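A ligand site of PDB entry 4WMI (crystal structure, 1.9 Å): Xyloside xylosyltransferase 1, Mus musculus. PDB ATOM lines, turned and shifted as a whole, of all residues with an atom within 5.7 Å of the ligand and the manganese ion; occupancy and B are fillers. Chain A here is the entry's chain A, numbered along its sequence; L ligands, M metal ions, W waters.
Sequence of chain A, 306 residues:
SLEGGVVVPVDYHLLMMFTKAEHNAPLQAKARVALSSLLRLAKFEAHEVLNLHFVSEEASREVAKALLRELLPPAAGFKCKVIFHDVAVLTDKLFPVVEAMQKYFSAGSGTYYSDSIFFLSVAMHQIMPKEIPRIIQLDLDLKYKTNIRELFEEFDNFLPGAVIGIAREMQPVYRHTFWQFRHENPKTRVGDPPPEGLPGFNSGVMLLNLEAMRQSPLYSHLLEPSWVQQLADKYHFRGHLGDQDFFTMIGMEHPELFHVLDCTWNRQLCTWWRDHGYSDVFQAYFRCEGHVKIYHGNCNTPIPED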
ATOM      1  N   MET A  16      -7.136  16.744 -17.488  1.00  0.00           N
ATOM      2  CA  MET A  16      -6.252  15.708 -18.010  1.00  0.00           C
ATOM      3  C   MET A  16      -6.792  14.329 -17.669  1.00  0.00           C
ATOM      4  O   MET A  16      -7.218  14.074 -16.531  1.00  0.00           O
ATOM      5  CB  MET A  16      -4.843  15.870 -17.449  1.00  0.00           C
ATOM      6  CG  MET A  16      -4.229  17.221 -17.824  1.00  0.00           C
ATOM      7  SD  MET A  16      -2.750  17.713 -16.945  1.00  0.00           S
ATOM      8  CE  MET A  16      -2.818  19.505 -17.133  1.00  0.00           C
ATOM      9  N   MET A  17      -6.716  13.441 -18.653  1.00  0.00           N
ATOM     10  CA  MET A  17      -6.972  12.026 -18.442  1.00  0.00           C
ATOM     11  C   MET A  17      -5.768  11.374 -17.781  1.00  0.00           C
ATOM     12  O   MET A  17      -4.646  11.535 -18.248  1.00  0.00           O
ATOM     13  CB  MET A  17      -7.210  11.331 -19.776  1.00  0.00           C
ATOM     14  CG  MET A  17      -8.399  11.847 -20.555  1.00  0.00           C
ATOM     15  SD  MET A  17      -9.924  11.391 -19.712  1.00  0.00           S
ATOM     16  CE  MET A  17      -9.619   9.642 -19.400  1.00  0.00           C
ATOM     17  N   PHE A  18      -5.985  10.640 -16.701  1.00  0.00           N
ATOM     18  CA  PHE A  18      -4.888   9.934 -16.032  1.00  0.00           C
ATOM     19  C   PHE A  18      -5.399   8.628 -15.470  1.00  0.00           C
ATOM     20  O   PHE A  18      -5.793   8.550 -14.307  1.00  0.00           O
ATOM     21  CB  PHE A  18      -4.274  10.783 -14.923  1.00  0.00           C
ATOM     22  CG  PHE A  18      -2.963  10.257 -14.384  1.00  0.00           C
ATOM     23  CD1 PHE A  18      -1.864  10.102 -15.230  1.00  0.00           C
ATOM     24  CD2 PHE A  18      -2.835   9.907 -13.047  1.00  0.00           C
ATOM     25  CE1 PHE A  18      -0.645   9.625 -14.733  1.00  0.00           C
ATOM     26  CE2 PHE A  18      -1.626   9.435 -12.542  1.00  0.00           C
ATOM     27  CZ  PHE A  18      -0.525   9.302 -13.389  1.00  0.00           C
ATOM     28  N   THR A  19      -5.423   7.609 -16.321  1.00  0.00           N
ATOM     29  CA  THR A  19      -6.043   6.335 -15.979  1.00  0.00           C
ATOM     30  C   THR A  19      -5.044   5.204 -16.166  1.00  0.00           C
ATOM     31  O   THR A  19      -4.102   5.300 -16.960  1.00  0.00           O
ATOM     32  CB  THR A  19      -7.254   6.037 -16.872  1.00  0.00           C
ATOM     33  OG1 THR A  19      -6.814   6.054 -18.239  1.00  0.00           O
ATOM     34  CG2 THR A  19      -8.349   7.086 -16.695  1.00  0.00           C
ATOM     35  N   LYS A  20      -5.296   4.101 -15.457  1.00  0.00           N
ATOM     36  CA  LYS A  20      -4.461   2.903 -15.537  1.00  0.00           C
ATOM     37  C   LYS A  20      -2.982   3.239 -15.322  1.00  0.00           C
ATOM     38  O   LYS A  20      -2.100   2.675 -15.965  1.00  0.00           O
ATOM     39  CB  LYS A  20      -4.670   2.205 -16.896  1.00  0.00           C
ATOM     40  CG  LYS A  20      -6.112   2.037 -17.331  1.00  0.00           C
ATOM     41  CD  LYS A  20      -6.820   0.948 -16.530  1.00  0.00           C
ATOM     42  CE  LYS A  20      -8.223   0.674 -17.057  1.00  0.00           C
ATOM     43  NZ  LYS A  20      -8.188   0.212 -18.477  1.00  0.00           N
ATOM     44  N   ASN A  24       2.383   1.637 -14.446  1.00  0.00           N
ATOM     45  CA  ASN A  24       2.583   2.122 -15.803  1.00  0.00           C
ATOM     46  C   ASN A  24       3.640   3.216 -15.726  1.00  0.00           C
ATOM     47  O   ASN A  24       3.340   4.416 -15.772  1.00  0.00           O
ATOM     48  CB  ASN A  24       1.276   2.643 -16.424  1.00  0.00           C
ATOM     49  CG  ASN A  24       1.404   2.964 -17.907  1.00  0.00           C
ATOM     50  OD1 ASN A  24       2.486   3.169 -18.446  1.00  0.00           O
ATOM     51  ND2 ASN A  24       0.263   3.018 -18.575  1.00  0.00           N
ATOM     52  N   LEU A  27       3.867   6.089 -18.448  1.00  0.00           N
ATOM     53  CA  LEU A  27       2.827   7.107 -18.278  1.00  0.00           C
ATOM     54  C   LEU A  27       3.105   8.055 -17.113  1.00  0.00           C
ATOM     55  O   LEU A  27       2.908   9.260 -17.228  1.00  0.00           O
ATOM     56  CB  LEU A  27       1.459   6.446 -18.084  1.00  0.00           C
ATOM     57  CG  LEU A  27       0.235   7.362 -17.913  1.00  0.00           C
ATOM     58  CD1 LEU A  27       0.006   8.205 -19.156  1.00  0.00           C
ATOM     59  CD2 LEU A  27      -0.999   6.520 -17.644  1.00  0.00           C
ATOM     60  N   LYS A  30       5.740  10.477 -18.198  1.00  0.00           N
ATOM     61  CA  LYS A  30       5.109  11.468 -19.074  1.00  0.00           C
ATOM     62  C   LYS A  30       4.390  12.521 -18.237  1.00  0.00           C
ATOM     63  O   LYS A  30       4.602  13.724 -18.414  1.00  0.00           O
ATOM     64  CB  LYS A  30       4.134  10.792 -20.031  1.00  0.00           C
ATOM     65  CG  LYS A  30       4.814  10.003 -21.126  1.00  0.00           C
ATOM     66  CD  LYS A  30       3.760   9.301 -21.967  1.00  0.00           C
ATOM     67  CE  LYS A  30       4.401   8.529 -23.103  1.00  0.00           C
ATOM     68  NZ  LYS A  30       3.370   7.794 -23.877  1.00  0.00           N
ATOM     69  N   VAL A  55      -9.123  12.946 -14.625  1.00  0.00           N
ATOM     70  CA  VAL A  55     -10.052  11.833 -14.786  1.00  0.00           C
ATOM     71  C   VAL A  55      -9.279  10.522 -14.591  1.00  0.00           C
ATOM     72  O   VAL A  55      -8.378  10.195 -15.357  1.00  0.00           O
ATOM     73  CB  VAL A  55     -10.749  11.871 -16.164  1.00  0.00           C
ATOM     74  CG1 VAL A  55     -11.790  10.758 -16.257  1.00  0.00           C
ATOM     75  CG2 VAL A  55     -11.416  13.214 -16.366  1.00  0.00           C
ATOM     76  N   PHE A 118     -12.967   7.957 -24.157  1.00  0.00           N
ATOM     77  CA  PHE A 118     -12.182   8.631 -25.201  1.00  0.00           C
ATOM     78  C   PHE A 118     -13.003   9.688 -25.966  1.00  0.00           C
ATOM     79  O   PHE A 118     -12.472  10.405 -26.791  1.00  0.00           O
ATOM     80  CB  PHE A 118     -11.504   7.614 -26.128  1.00  0.00           C
ATOM     81  CG  PHE A 118     -10.621   6.651 -25.381  1.00  0.00           C
ATOM     82  CD1 PHE A 118      -9.503   7.110 -24.685  1.00  0.00           C
ATOM     83  CD2 PHE A 118     -10.938   5.291 -25.328  1.00  0.00           C
ATOM     84  CE1 PHE A 118      -8.694   6.230 -23.966  1.00  0.00           C
ATOM     85  CE2 PHE A 118     -10.124   4.410 -24.629  1.00  0.00           C
ATOM     86  CZ  PHE A 118      -9.004   4.869 -23.943  1.00  0.00           C
ATOM     87  N   LEU A 138      -5.983  18.604 -21.922  1.00  0.00           N
ATOM     88  CA  LEU A 138      -4.576  18.422 -22.310  1.00  0.00           C
ATOM     89  C   LEU A 138      -4.146  16.987 -22.108  1.00  0.00           C
ATOM     90  O   LEU A 138      -4.487  16.357 -21.098  1.00  0.00           O
ATOM     91  CB  LEU A 138      -3.681  19.348 -21.477  1.00  0.00           C
ATOM     92  CG  LEU A 138      -4.012  20.843 -21.585  1.00  0.00           C
ATOM     93  CD1 LEU A 138      -3.691  21.598 -20.295  1.00  0.00           C
ATOM     94  CD2 LEU A 138      -3.284  21.450 -22.774  1.00  0.00           C
ATOM     95  N   ASP A 139      -3.366  16.486 -23.072  1.00  0.00           N
ATOM     96  CA  ASP A 139      -2.707  15.180 -22.944  1.00  0.00           C
ATOM     97  C   ASP A 139      -1.623  15.286 -21.861  1.00  0.00           C
ATOM     98  O   ASP A 139      -1.231  16.375 -21.472  1.00  0.00           O
ATOM     99  CB  ASP A 139      -2.070  14.772 -24.280  1.00  0.00           C
ATOM    100  CG  ASP A 139      -3.041  14.055 -25.206  1.00  0.00           C
ATOM    101  OD1 ASP A 139      -4.262  14.069 -24.927  1.00  0.00           O
ATOM    102  OD2 ASP A 139      -2.588  13.496 -26.212  1.00  0.00           O
ATOM    103  N   LEU A 140      -1.166  14.139 -21.371  1.00  0.00           N
ATOM    104  CA  LEU A 140      -0.086  14.121 -20.399  1.00  0.00           C
ATOM    105  C   LEU A 140       1.302  13.870 -20.995  1.00  0.00           C
ATOM    106  O   LEU A 140       2.305  13.858 -20.287  1.00  0.00           O
ATOM    107  CB  LEU A 140      -0.398  13.174 -19.224  1.00  0.00           C
ATOM    108  CG  LEU A 140      -1.302  13.828 -18.146  1.00  0.00           C
ATOM    109  CD1 LEU A 140      -1.818  12.814 -17.150  1.00  0.00           C
ATOM    110  CD2 LEU A 140      -0.590  14.953 -17.389  1.00  0.00           C
ATOM    111  N   ASP A 141       1.363  13.662 -22.310  1.00  0.00           N
ATOM    112  CA  ASP A 141       2.658  13.499 -22.990  1.00  0.00           C
ATOM    113  C   ASP A 141       3.057  14.806 -23.690  1.00  0.00           C
ATOM    114  O   ASP A 141       3.480  14.797 -24.845  1.00  0.00           O
ATOM    115  CB  ASP A 141       2.618  12.343 -23.985  1.00  0.00           C
ATOM    116  CG  ASP A 141       1.532  12.493 -25.042  1.00  0.00           C
ATOM    117  OD1 ASP A 141       0.538  13.206 -24.806  1.00  0.00           O
ATOM    118  OD2 ASP A 141       1.642  11.862 -26.104  1.00  0.00           O
ATOM    119  N   LEU A 142       2.896  15.903 -22.964  1.00  0.00           N
ATOM    120  CA  LEU A 142       3.207  17.243 -23.408  1.00  0.00           C
ATOM    121  C   LEU A 142       4.384  17.759 -22.607  1.00  0.00           C
ATOM    122  O   LEU A 142       4.712  17.218 -21.551  1.00  0.00           O
ATOM    123  CB  LEU A 142       2.011  18.174 -23.210  1.00  0.00           C
ATOM    124  CG  LEU A 142       0.673  17.832 -23.885  1.00  0.00           C
ATOM    125  CD1 LEU A 142      -0.342  18.924 -23.578  1.00  0.00           C
ATOM    126  CD2 LEU A 142       0.896  17.759 -25.382  1.00  0.00           C
ATOM    127  N   GLY A 204      -4.604  16.542 -28.632  1.00  0.00           N
ATOM    128  CA  GLY A 204      -3.730  16.715 -27.454  1.00  0.00           C
ATOM    129  C   GLY A 204      -3.917  17.994 -26.655  1.00  0.00           C
ATOM    130  O   GLY A 204      -3.560  18.051 -25.468  1.00  0.00           O
ATOM    131  N   LEU A 241      -9.379   6.695 -32.996  1.00  0.00           N
ATOM    132  CA  LEU A 241      -8.839   7.784 -32.164  1.00  0.00           C
ATOM    133  C   LEU A 241      -9.862   8.628 -31.403  1.00  0.00           C
ATOM    134  O   LEU A 241      -9.513   9.675 -30.838  1.00  0.00           O
ATOM    135  CB  LEU A 241      -7.881   8.681 -32.998  1.00  0.00           C
ATOM    136  CG  LEU A 241      -6.713   7.923 -33.635  1.00  0.00           C
ATOM    137  CD1 LEU A 241      -5.748   8.843 -34.396  1.00  0.00           C
ATOM    138  CD2 LEU A 241      -5.968   7.155 -32.552  1.00  0.00           C
ATOM    139  N   HIS A 296       4.431  18.025 -28.076  1.00  0.00           N
ATOM    140  CA  HIS A 296       3.566  16.879 -27.883  1.00  0.00           C
ATOM    141  C   HIS A 296       4.282  15.633 -28.348  1.00  0.00           C
ATOM    142  O   HIS A 296       4.401  15.366 -29.557  1.00  0.00           O
ATOM    143  CB  HIS A 296       2.255  17.105 -28.654  1.00  0.00           C
ATOM    144  CG  HIS A 296       1.192  16.046 -28.405  1.00  0.00           C
ATOM    145  ND1 HIS A 296      -0.013  16.075 -29.025  1.00  0.00           N
ATOM    146  CD2 HIS A 296       1.187  14.914 -27.598  1.00  0.00           C
ATOM    147  CE1 HIS A 296      -0.744  15.011 -28.620  1.00  0.00           C
ATOM    148  NE2 HIS A 296      -0.009  14.308 -27.735  1.00  0.00           N
ATOM    149  N   GLY A 297       4.757  14.851 -27.377  1.00  0.00           N
ATOM    150  CA  GLY A 297       5.517  13.641 -27.679  1.00  0.00           C
ATOM    151  C   GLY A 297       4.567  12.508 -27.957  1.00  0.00           C
ATOM    152  O   GLY A 297       4.583  11.491 -27.240  1.00  0.00           O
ATOM    153  N   ASN A 298       3.717  12.665 -28.981  1.00  0.00           N
ATOM    154  CA  ASN A 298       2.776  11.589 -29.299  1.00  0.00           C
ATOM    155  C   ASN A 298       3.423  10.327 -29.872  1.00  0.00           C
ATOM    156  O   ASN A 298       4.597  10.317 -30.243  1.00  0.00           O
ATOM    157  CB  ASN A 298       1.491  12.055 -30.058  1.00  0.00           C
ATOM    158  CG  ASN A 298       1.759  12.701 -31.433  1.00  0.00           C
ATOM    159  OD1 ASN A 298       0.884  12.658 -32.316  1.00  0.00           O
ATOM    160  ND2 ASN A 298       2.892  13.345 -31.587  1.00  0.00           N
ATOM    161  N   CYS A 299       2.632   9.269 -29.910  1.00  0.00           N
ATOM    162  CA  CYS A 299       3.070   7.897 -30.189  1.00  0.00           C
ATOM    163  C   CYS A 299       4.392   7.554 -29.466  1.00  0.00           C
ATOM    164  O   CYS A 299       5.343   7.038 -30.074  1.00  0.00           O
ATOM    165  CB  CYS A 299       3.070   7.560 -31.691  1.00  0.00           C
ATOM    166  SG  CYS A 299       4.427   8.219 -32.708  1.00  0.00           S
ATOM    167  N   ASN A 300       4.430   7.871 -28.181  1.00  0.00           N
ATOM    168  CA  ASN A 300       5.580   7.555 -27.322  1.00  0.00           C
ATOM    169  C   ASN A 300       6.901   8.140 -27.823  1.00  0.00           C
ATOM    170  O   ASN A 300       7.945   7.542 -27.609  1.00  0.00           O
ATOM    171  CB  ASN A 300       5.724   6.040 -27.184  1.00  0.00           C
ATOM    172  CG  ASN A 300       4.486   5.399 -26.622  1.00  0.00           C
ATOM    173  OD1 ASN A 300       3.970   5.843 -25.607  1.00  0.00           O
ATOM    174  ND2 ASN A 300       3.991   4.369 -27.291  1.00  0.00           N
HETATM  175  N1  LIG L   1      -3.969   8.126 -21.189  1.00  0.00           N
HETATM  176  C1  LIG L   1      -4.088   7.599 -19.885  1.00  0.00           C
HETATM  177  N2  LIG L   1      -3.870   6.297 -19.651  1.00  0.00           N
HETATM  178  C2  LIG L   1      -3.555   5.493 -20.664  1.00  0.00           C
HETATM  179  C3  LIG L   1      -3.422   5.966 -21.974  1.00  0.00           C
HETATM  180  C4  LIG L   1      -3.644   7.317 -22.210  1.00  0.00           C
HETATM  181  O1  LIG L   1      -4.406   8.367 -18.954  1.00  0.00           O
HETATM  182  O2  LIG L   1      -3.360   4.288 -20.437  1.00  0.00           O
HETATM  183  C5  LIG L   1      -4.244   9.563 -21.386  1.00  0.00           C
HETATM  184  C6  LIG L   1      -3.007  10.422 -21.214  1.00  0.00           C
HETATM  185  O3  LIG L   1      -3.431  11.702 -20.725  1.00  0.00           O
HETATM  186  C7  LIG L   1      -2.512  10.600 -22.643  1.00  0.00           C
HETATM  187  C8  LIG L   1      -3.812  10.614 -23.459  1.00  0.00           C
HETATM  188  O4  LIG L   1      -4.721   9.802 -22.707  1.00  0.00           O
HETATM  189  O5  LIG L   1      -1.732  11.789 -22.773  1.00  0.00           O
HETATM  190  C9  LIG L   1      -3.709  10.017 -24.861  1.00  0.00           C
HETATM  191  O6  LIG L   1      -2.730   8.972 -24.891  1.00  0.00           O
HETATM  192  P1  LIG L   1      -1.259   9.298 -25.436  1.00  0.00           P
HETATM  193  O7  LIG L   1      -1.033  10.768 -25.172  1.00  0.00           O
HETATM  194  O8  LIG L   1      -0.262   8.273 -24.928  1.00  0.00           O
HETATM  195  O9  LIG L   1      -1.518   9.004 -26.997  1.00  0.00           O
HETATM  196  P2  LIG L   1      -1.173   9.953 -28.256  1.00  0.00           P
HETATM  197  O10 LIG L   1      -2.481   9.770 -28.948  1.00  0.00           O
HETATM  198  O11 LIG L   1      -0.058   9.249 -28.988  1.00  0.00           O
HETATM  199  O12 LIG L   1      -0.926  11.390 -27.813  1.00  0.00           O
HETATM  200 MN    MN M   1      -0.610  12.667 -26.553  1.00  0.00          MN
HETATM  201  O   HOH W   1      -5.616  14.058 -21.090  1.00  0.00           O
HETATM  202  O   HOH W   2       2.594   9.300 -26.300  1.00  0.00           O
HETATM  203  O   HOH W   3       0.401   6.814 -28.282  1.00  0.00           O
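NZ of Lys 30 is in hydrogen-bond range of OD1 of Asn 300, at 2.7 Å.
The backbone NH of Phe 18 lies within hydrogen-bond range of the backbone carbonyl oxygen of Val 55, 2.8 Å away.
The backbone carbonyl oxygen (O) of His 296 sits at hydrogen-bond distance from the side-chain amide nitrogen (ND2) of Asn 298, at 3.2 Å.
O of Gly 204 is in hydrogen-bond range of N of Asp 139 (2.9 Å).
The backbone carbonyl oxygen (O) of Asp 141 is in hydrogen-bond range of the backbone NH (N) of Gly 297 (2.8 Å).
N of Leu 27 is in hydrogen-bond range of OD1 of Asn 24 (3.2 Å).
The manganese ion is bound by an oxygen (O12) of the ligand (1.8 Å), a ring nitrogen (NE2) of His 296 (2.1 Å), the side-chain carboxylate (OD1) of Asp 141 (2.2 Å), the side-chain carboxylate (OD2) of Asp 139 (2.2 Å), an oxygen (O7) of the ligand (2.4 Å) and the side-chain carboxylate (OD2) of Asp 141 (2.4 Å).
The manganese ion has six donor atoms within binding distance.
Merely in contact with the ligand: Phe 18 (3.4 Å), Leu 27 (3.5 Å) and Asn 298 (3.4 Å).
Within 4 Å of the ligand: Met 17, Phe 18, Thr 19, Leu 27, Lys 30, Asp 139, Leu 140, Asp 141, His 296, Asn 298 and Cys 299.
The nearest printed residue that does not touch the ligand is Asn 24 (4.3 Å).
Water W1 lies within hydrogen-bond range of O of Leu 138 (2.6 Å), N of Met 17 (2.7 Å) and O3 of the ligand (3.2 Å).
Water W2 lies within hydrogen-bond range of the side-chain amino group (NZ) of Lys 30 (3.0 Å), the backbone NH (N) of Asn 300 (3.0 Å), the backbone carbonyl oxygen (O) of Gly 297 (3.1 Å) and an oxygen (O8) of the ligand (3.3 Å).
Three residues have an atom within 4 Å of the manganese ion: Asp 139, Asp 141 and His 296.
The nearest printed residue that does not touch the manganese ion is Asn 298 (4.1 Å).
The backbone NH (N) of Cys 299 lies within hydrogen-bond range of an oxygen (O11) of the ligand (2.8 Å).
O8 of the ligand is in salt-bridge range of NZ of Lys 30 (3.8 Å).
An oxygen (O1) of the ligand sits at hydrogen-bond distance from the backbone NH (N) of Thr 19 (2.9 Å).
The backbone carbonyl oxygen (O) of Met 17 is in hydrogen-bond range of an oxygen (O3) of the ligand, at 2.8 Å.
The backbone NH of Leu 140 lies within hydrogen-bond range of an oxygen (O5) of the ligand (2.8 Å).
The backbone carbonyl oxygen of Thr 19 is in hydrogen-bond range of a nitrogen (N2) of the ligand (2.9 Å).
A nitrogen (N2) of the ligand lies within hydrogen-bond range of the side-chain hydroxyl of Thr 19 (3.3 Å).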
